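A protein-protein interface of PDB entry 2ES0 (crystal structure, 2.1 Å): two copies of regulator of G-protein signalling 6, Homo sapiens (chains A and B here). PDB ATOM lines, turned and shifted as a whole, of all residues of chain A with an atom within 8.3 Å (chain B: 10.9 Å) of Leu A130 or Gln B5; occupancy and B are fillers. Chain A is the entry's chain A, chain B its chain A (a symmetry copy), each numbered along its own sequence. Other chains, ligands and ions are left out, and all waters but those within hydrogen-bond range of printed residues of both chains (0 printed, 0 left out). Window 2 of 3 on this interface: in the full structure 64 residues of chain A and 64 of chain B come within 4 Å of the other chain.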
ATOM      1  N   TYR A 125     -21.144  34.475 -17.820  1.00  0.00           N
ATOM      2  CA  TYR A 125     -21.067  33.048 -17.484  1.00  0.00           C
ATOM      3  C   TYR A 125     -20.309  32.795 -16.179  1.00  0.00           C
ATOM      4  O   TYR A 125     -20.845  32.177 -15.257  1.00  0.00           O
ATOM      5  CB  TYR A 125     -20.399  32.258 -18.616  1.00  0.00           C
ATOM      6  CG  TYR A 125     -20.234  30.783 -18.314  1.00  0.00           C
ATOM      7  CD1 TYR A 125     -21.316  29.913 -18.392  1.00  0.00           C
ATOM      8  CD2 TYR A 125     -18.999  30.260 -17.942  1.00  0.00           C
ATOM      9  CE1 TYR A 125     -21.173  28.558 -18.114  1.00  0.00           C
ATOM     10  CE2 TYR A 125     -18.842  28.907 -17.661  1.00  0.00           C
ATOM     11  CZ  TYR A 125     -19.931  28.061 -17.749  1.00  0.00           C
ATOM     12  OH  TYR A 125     -19.781  26.721 -17.473  1.00  0.00           O
ATOM     13  N   GLN A 126     -19.067  33.271 -16.115  1.00  0.00           N
ATOM     14  CA  GLN A 126     -18.177  33.001 -14.975  1.00  0.00           C
ATOM     15  C   GLN A 126     -18.776  33.445 -13.637  1.00  0.00           C
ATOM     16  O   GLN A 126     -18.567  32.791 -12.619  1.00  0.00           O
ATOM     17  CB  GLN A 126     -16.808  33.664 -15.183  1.00  0.00           C
ATOM     18  CG  GLN A 126     -16.000  33.103 -16.358  1.00  0.00           C
ATOM     19  CD  GLN A 126     -15.490  31.688 -16.125  1.00  0.00           C
ATOM     20  OE1 GLN A 126     -15.055  31.344 -15.025  1.00  0.00           O
ATOM     21  NE2 GLN A 126     -15.523  30.865 -17.169  1.00  0.00           N
ATOM     22  N   ASP A 127     -19.529  34.545 -13.648  1.00  0.00           N
ATOM     23  CA  ASP A 127     -20.236  35.022 -12.450  1.00  0.00           C
ATOM     24  C   ASP A 127     -21.257  34.002 -11.922  1.00  0.00           C
ATOM     25  O   ASP A 127     -21.539  33.975 -10.722  1.00  0.00           O
ATOM     26  CB  ASP A 127     -20.940  36.364 -12.718  1.00  0.00           C
ATOM     27  CG  ASP A 127     -19.959  37.517 -12.954  1.00  0.00           C
ATOM     28  OD1 ASP A 127     -18.868  37.529 -12.337  1.00  0.00           O
ATOM     29  OD2 ASP A 127     -20.289  38.421 -13.759  1.00  0.00           O
ATOM     30  N   LEU A 128     -21.803  33.173 -12.812  1.00  0.00           N
ATOM     31  CA  LEU A 128     -22.709  32.090 -12.408  1.00  0.00           C
ATOM     32  C   LEU A 128     -21.961  30.966 -11.688  1.00  0.00           C
ATOM     33  O   LEU A 128     -22.516  30.324 -10.793  1.00  0.00           O
ATOM     34  CB  LEU A 128     -23.443  31.498 -13.615  1.00  0.00           C
ATOM     35  CG  LEU A 128     -24.146  32.457 -14.575  1.00  0.00           C
ATOM     36  CD1 LEU A 128     -24.797  31.677 -15.707  1.00  0.00           C
ATOM     37  CD2 LEU A 128     -25.171  33.313 -13.852  1.00  0.00           C
ATOM     38  N   LEU A 129     -20.706  30.732 -12.075  1.00  0.00           N
ATOM     39  CA  LEU A 129     -19.933  29.596 -11.550  1.00  0.00           C
ATOM     40  C   LEU A 129     -19.550  29.697 -10.068  1.00  0.00           C
ATOM     41  O   LEU A 129     -18.898  28.794  -9.547  1.00  0.00           O
ATOM     42  CB  LEU A 129     -18.685  29.310 -12.410  1.00  0.00           C
ATOM     43  CG  LEU A 129     -18.842  28.243 -13.503  1.00  0.00           C
ATOM     44  CD1 LEU A 129     -17.495  27.984 -14.167  1.00  0.00           C
ATOM     45  CD2 LEU A 129     -19.417  26.935 -12.954  1.00  0.00           C
ATOM     46  N   LEU A 130     -19.934  30.787  -9.402  1.00  0.00           N
ATOM     47  CA  LEU A 130     -20.081  30.794  -7.941  1.00  0.00           C
ATOM     48  C   LEU A 130     -21.013  31.926  -7.503  1.00  0.00           C
ATOM     49  O   LEU A 130     -22.198  31.937  -7.848  1.00  0.00           O
ATOM     50  CB  LEU A 130     -18.725  30.912  -7.228  1.00  0.00           C
ATOM     51  CG  LEU A 130     -17.915  29.636  -6.954  1.00  0.00           C
ATOM     52  CD1 LEU A 130     -16.633  29.989  -6.216  1.00  0.00           C
ATOM     53  CD2 LEU A 130     -18.715  28.591  -6.169  1.00  0.00           C
ATOM     54  N   MET B   2     -31.948  29.932  -8.641  1.00  0.00           N
ATOM     55  CA  MET B   2     -30.802  29.889  -9.599  1.00  0.00           C
ATOM     56  C   MET B   2     -30.678  28.462 -10.146  1.00  0.00           C
ATOM     57  O   MET B   2     -31.364  27.550  -9.663  1.00  0.00           O
ATOM     58  CB  MET B   2     -29.507  30.303  -8.878  1.00  0.00           C
ATOM     59  CG  MET B   2     -28.606  31.283  -9.638  1.00  0.00           C
ATOM     60  N   PRO B   3     -29.820  28.259 -11.168  1.00  0.00           N
ATOM     61  CA  PRO B   3     -29.472  26.897 -11.566  1.00  0.00           C
ATOM     62  C   PRO B   3     -28.258  26.401 -10.780  1.00  0.00           C
ATOM     63  O   PRO B   3     -27.444  27.208 -10.320  1.00  0.00           O
ATOM     64  CB  PRO B   3     -29.152  27.033 -13.064  1.00  0.00           C
ATOM     65  CG  PRO B   3     -28.999  28.522 -13.328  1.00  0.00           C
ATOM     66  CD  PRO B   3     -29.134  29.245 -12.020  1.00  0.00           C
ATOM     67  N   SER B   4     -28.138  25.086 -10.625  1.00  0.00           N
ATOM     68  CA  SER B   4     -27.060  24.504  -9.826  1.00  0.00           C
ATOM     69  C   SER B   4     -25.711  24.660 -10.511  1.00  0.00           C
ATOM     70  O   SER B   4     -25.633  24.931 -11.709  1.00  0.00           O
ATOM     71  CB  SER B   4     -27.314  23.019  -9.584  1.00  0.00           C
ATOM     72  OG  SER B   4     -27.160  22.288 -10.790  1.00  0.00           O
ATOM     73  N   GLN B   5     -24.650  24.456  -9.738  1.00  0.00           N
ATOM     74  CA  GLN B   5     -23.294  24.475 -10.269  1.00  0.00           C
ATOM     75  C   GLN B   5     -23.069  23.313 -11.231  1.00  0.00           C
ATOM     76  O   GLN B   5     -22.318  23.439 -12.198  1.00  0.00           O
ATOM     77  CB  GLN B   5     -22.271  24.415  -9.131  1.00  0.00           C
ATOM     78  CG  GLN B   5     -22.363  25.571  -8.143  1.00  0.00           C
ATOM     79  CD  GLN B   5     -22.070  26.915  -8.784  1.00  0.00           C
ATOM     80  OE1 GLN B   5     -20.961  27.428  -8.667  1.00  0.00           O
ATOM     81  NE2 GLN B   5     -23.060  27.490  -9.465  1.00  0.00           N
ATOM     82  N   GLN B   6     -23.731  22.188 -10.966  1.00  0.00           N
ATOM     83  CA  GLN B   6     -23.582  21.001 -11.790  1.00  0.00           C
ATOM     84  C   GLN B   6     -24.035  21.264 -13.229  1.00  0.00           C
ATOM     85  O   GLN B   6     -23.339  20.878 -14.169  1.00  0.00           O
ATOM     86  CB  GLN B   6     -24.362  19.830 -11.188  1.00  0.00           C
ATOM     87  CG  GLN B   6     -24.159  18.504 -11.912  1.00  0.00           C
ATOM     88  N   ARG B   7     -25.186  21.922 -13.398  1.00  0.00           N
ATOM     89  CA  ARG B   7     -25.704  22.204 -14.743  1.00  0.00           C
ATOM     90  C   ARG B   7     -25.013  23.417 -15.374  1.00  0.00           C
ATOM     91  O   ARG B   7     -24.697  23.393 -16.560  1.00  0.00           O
ATOM     92  CB  ARG B   7     -27.242  22.331 -14.765  1.00  0.00           C
ATOM     93  CG  ARG B   7     -27.832  23.661 -14.289  1.00  0.00           C
ATOM     94  CD  ARG B   7     -29.369  23.567 -14.080  1.00  0.00           C
ATOM     95  NE  ARG B   7     -30.169  23.923 -15.258  1.00  0.00           N
ATOM     96  CZ  ARG B   7     -31.499  24.072 -15.254  1.00  0.00           C
ATOM     97  NH1 ARG B   7     -32.211  23.900 -14.146  1.00  0.00           N
ATOM     98  NH2 ARG B   7     -32.134  24.406 -16.372  1.00  0.00           N
ATOM     99  N   VAL B   8     -24.750  24.452 -14.578  1.00  0.00           N
ATOM    100  CA  VAL B   8     -23.947  25.590 -15.038  1.00  0.00           C
ATOM    101  C   VAL B   8     -22.603  25.098 -15.603  1.00  0.00           C
ATOM    102  O   VAL B   8     -22.148  25.571 -16.647  1.00  0.00           O
ATOM    103  CB  VAL B   8     -23.734  26.651 -13.921  1.00  0.00           C
ATOM    104  CG1 VAL B   8     -22.703  27.696 -14.341  1.00  0.00           C
ATOM    105  CG2 VAL B   8     -25.054  27.345 -13.584  1.00  0.00           C
ATOM    106  N   LYS B   9     -21.997  24.129 -14.924  1.00  0.00           N
ATOM    107  CA  LYS B   9     -20.778  23.480 -15.406  1.00  0.00           C
ATOM    108  C   LYS B   9     -21.011  22.677 -16.693  1.00  0.00           C
ATOM    109  O   LYS B   9     -20.142  22.647 -17.562  1.00  0.00           O
ATOM    110  CB  LYS B   9     -20.200  22.567 -14.321  1.00  0.00           C
ATOM    111  CG  LYS B   9     -18.803  22.038 -14.612  1.00  0.00           C
ATOM    112  N   ARG B  10     -22.177  22.036 -16.816  1.00  0.00           N
ATOM    113  CA  ARG B  10     -22.475  21.194 -17.983  1.00  0.00           C
ATOM    114  C   ARG B  10     -22.582  22.018 -19.267  1.00  0.00           C
ATOM    115  O   ARG B  10     -22.258  21.531 -20.352  1.00  0.00           O
ATOM    116  CB  ARG B  10     -23.763  20.377 -17.782  1.00  0.00           C
ATOM    117  CG  ARG B  10     -23.757  19.041 -18.540  1.00  0.00           C
ATOM    118  CD  ARG B  10     -25.051  18.216 -18.388  1.00  0.00           C
ATOM    119  NE  ARG B  10     -25.896  18.620 -17.257  1.00  0.00           N
ATOM    120  CZ  ARG B  10     -25.760  18.210 -15.996  1.00  0.00           C
ATOM    121  NH1 ARG B  10     -24.793  17.363 -15.637  1.00  0.00           N
ATOM    122  NH2 ARG B  10     -26.601  18.666 -15.069  1.00  0.00           N
ATOM    123  N   TRP B  11     -23.039  23.259 -19.141  1.00  0.00           N
ATOM    124  CA  TRP B  11     -23.076  24.176 -20.274  1.00  0.00           C
ATOM    125  C   TRP B  11     -21.677  24.365 -20.870  1.00  0.00           C
ATOM    126  O   TRP B  11     -21.530  24.525 -22.079  1.00  0.00           O
ATOM    127  CB  TRP B  11     -23.638  25.540 -19.867  1.00  0.00           C
ATOM    128  CG  TRP B  11     -24.988  25.497 -19.225  1.00  0.00           C
ATOM    129  CD1 TRP B  11     -25.879  24.459 -19.237  1.00  0.00           C
ATOM    130  CD2 TRP B  11     -25.611  26.552 -18.483  1.00  0.00           C
ATOM    131  NE1 TRP B  11     -27.005  24.798 -18.535  1.00  0.00           N
ATOM    132  CE2 TRP B  11     -26.872  26.076 -18.061  1.00  0.00           C
ATOM    133  CE3 TRP B  11     -25.225  27.855 -18.133  1.00  0.00           C
ATOM    134  CZ2 TRP B  11     -27.756  26.857 -17.310  1.00  0.00           C
ATOM    135  CZ3 TRP B  11     -26.099  28.633 -17.385  1.00  0.00           C
ATOM    136  CH2 TRP B  11     -27.351  28.129 -16.976  1.00  0.00           C
ATOM    137  N   GLY B  12     -20.655  24.341 -20.018  1.00  0.00           N
ATOM    138  CA  GLY B  12     -19.274  24.449 -20.472  1.00  0.00           C
ATOM    139  C   GLY B  12     -18.642  23.138 -20.913  1.00  0.00           C
ATOM    140  O   GLY B  12     -17.420  23.070 -21.102  1.00  0.00           O
ATOM    141  N   PHE B  13     -19.457  22.096 -21.067  1.00  0.00           N
ATOM    142  CA  PHE B  13     -18.957  20.782 -21.465  1.00  0.00           C
ATOM    143  C   PHE B  13     -18.952  20.704 -22.979  1.00  0.00           C
ATOM    144  O   PHE B  13     -17.997  20.228 -23.588  1.00  0.00           O
ATOM    145  CB  PHE B  13     -19.830  19.663 -20.884  1.00  0.00           C
ATOM    146  CG  PHE B  13     -19.255  18.290 -21.068  1.00  0.00           C
ATOM    147  CD1 PHE B  13     -18.336  17.782 -20.156  1.00  0.00           C
ATOM    148  CD2 PHE B  13     -19.624  17.506 -22.157  1.00  0.00           C
ATOM    149  CE1 PHE B  13     -17.795  16.509 -20.325  1.00  0.00           C
ATOM    150  CE2 PHE B  13     -19.087  16.234 -22.336  1.00  0.00           C
ATOM    151  CZ  PHE B  13     -18.172  15.735 -21.417  1.00  0.00           C
ATOM    152  N   ASP B  21     -30.381  22.765 -22.908  1.00  0.00           N
ATOM    153  CA  ASP B  21     -30.920  23.269 -21.657  1.00  0.00           C
ATOM    154  C   ASP B  21     -31.447  24.687 -21.868  1.00  0.00           C
ATOM    155  O   ASP B  21     -30.678  25.597 -22.179  1.00  0.00           O
ATOM    156  CB  ASP B  21     -29.828  23.209 -20.587  1.00  0.00           C
ATOM    157  CG  ASP B  21     -30.274  23.748 -19.252  1.00  0.00           C
ATOM    158  OD1 ASP B  21     -31.225  24.559 -19.186  1.00  0.00           O
ATOM    159  OD2 ASP B  21     -29.637  23.367 -18.255  1.00  0.00           O
ATOM    160  N   VAL B  23     -32.523  27.014 -19.918  1.00  0.00           N
ATOM    161  CA  VAL B  23     -32.014  28.068 -19.043  1.00  0.00           C
ATOM    162  C   VAL B  23     -30.594  28.495 -19.459  1.00  0.00           C
ATOM    163  O   VAL B  23     -30.260  29.676 -19.382  1.00  0.00           O
ATOM    164  CB  VAL B  23     -32.058  27.655 -17.541  1.00  0.00           C
ATOM    165  CG1 VAL B  23     -31.363  28.696 -16.650  1.00  0.00           C
ATOM    166  CG2 VAL B  23     -33.502  27.468 -17.095  1.00  0.00           C
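The backbone carbonyl oxygen of Leu A128 is in hydrogen-bond range of the side-chain amide nitrogen of Gln B5 (3.2 Å).
OH of Tyr A125 sits at hydrogen-bond distance from O of Val B8, at 2.8 Å.
The backbone carbonyl oxygen (O) of Leu A129 sits close to the side-chain amide oxygen (OE1) of Gln B5 (2.6 Å).
The indole nitrogen (NE1) of Trp B11 lies within hydrogen-bond range of the side-chain carboxylate (OD2) of Asp B21, at 3.0 Å.
O of Arg B7 sits close to NE1 of Trp B11.
Among the printed residues, merely in contact across the chains: Tyr A125 with Lys B9 (3.97 Å), Tyr A125 with Gly B12 (3.6 Å), Leu A128 with Val B8 (3.9 Å), Leu A128 with Trp B11 (3.7 Å), Leu A129 with Val B8 (3.6 Å) and Leu A130 with Gln B5 (3.6 Å).
Gln B5 touches three residues of chain A.
Leu A129 touches two residues of chain B.
No residue of chain A comes within 4 Å of Ser B4.
Printed residues of chain B within 4 Å of Tyr A125: Val B8 (2.8 Å), Lys B9 (3.97 Å) and Gly B12 (3.6 Å).
Printed residues of chain A within 4 Å of Trp B11: Leu A128.
Of the 6 printed residues of chain A, 4 touch a printed residue of chain B.
Printed residues of chain A that touch a printed residue of chain B: Tyr A125, Leu A128, Leu A129 and Leu A130.
Hydrophobic or aromatic side chains of chain A within 4 Å of the printed part of chain B: Tyr A125, Leu A128, Leu A129 and Leu A130.
Among the printed residues, no Asp or Glu carboxylate lies within 4 Å of a Lys or Arg side-chain nitrogen of the other chain.
No position is printed for both chains.
Of the 9 pairs that touch across the chains among the printed residues, none has its exchanged pair printed and touching as well.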
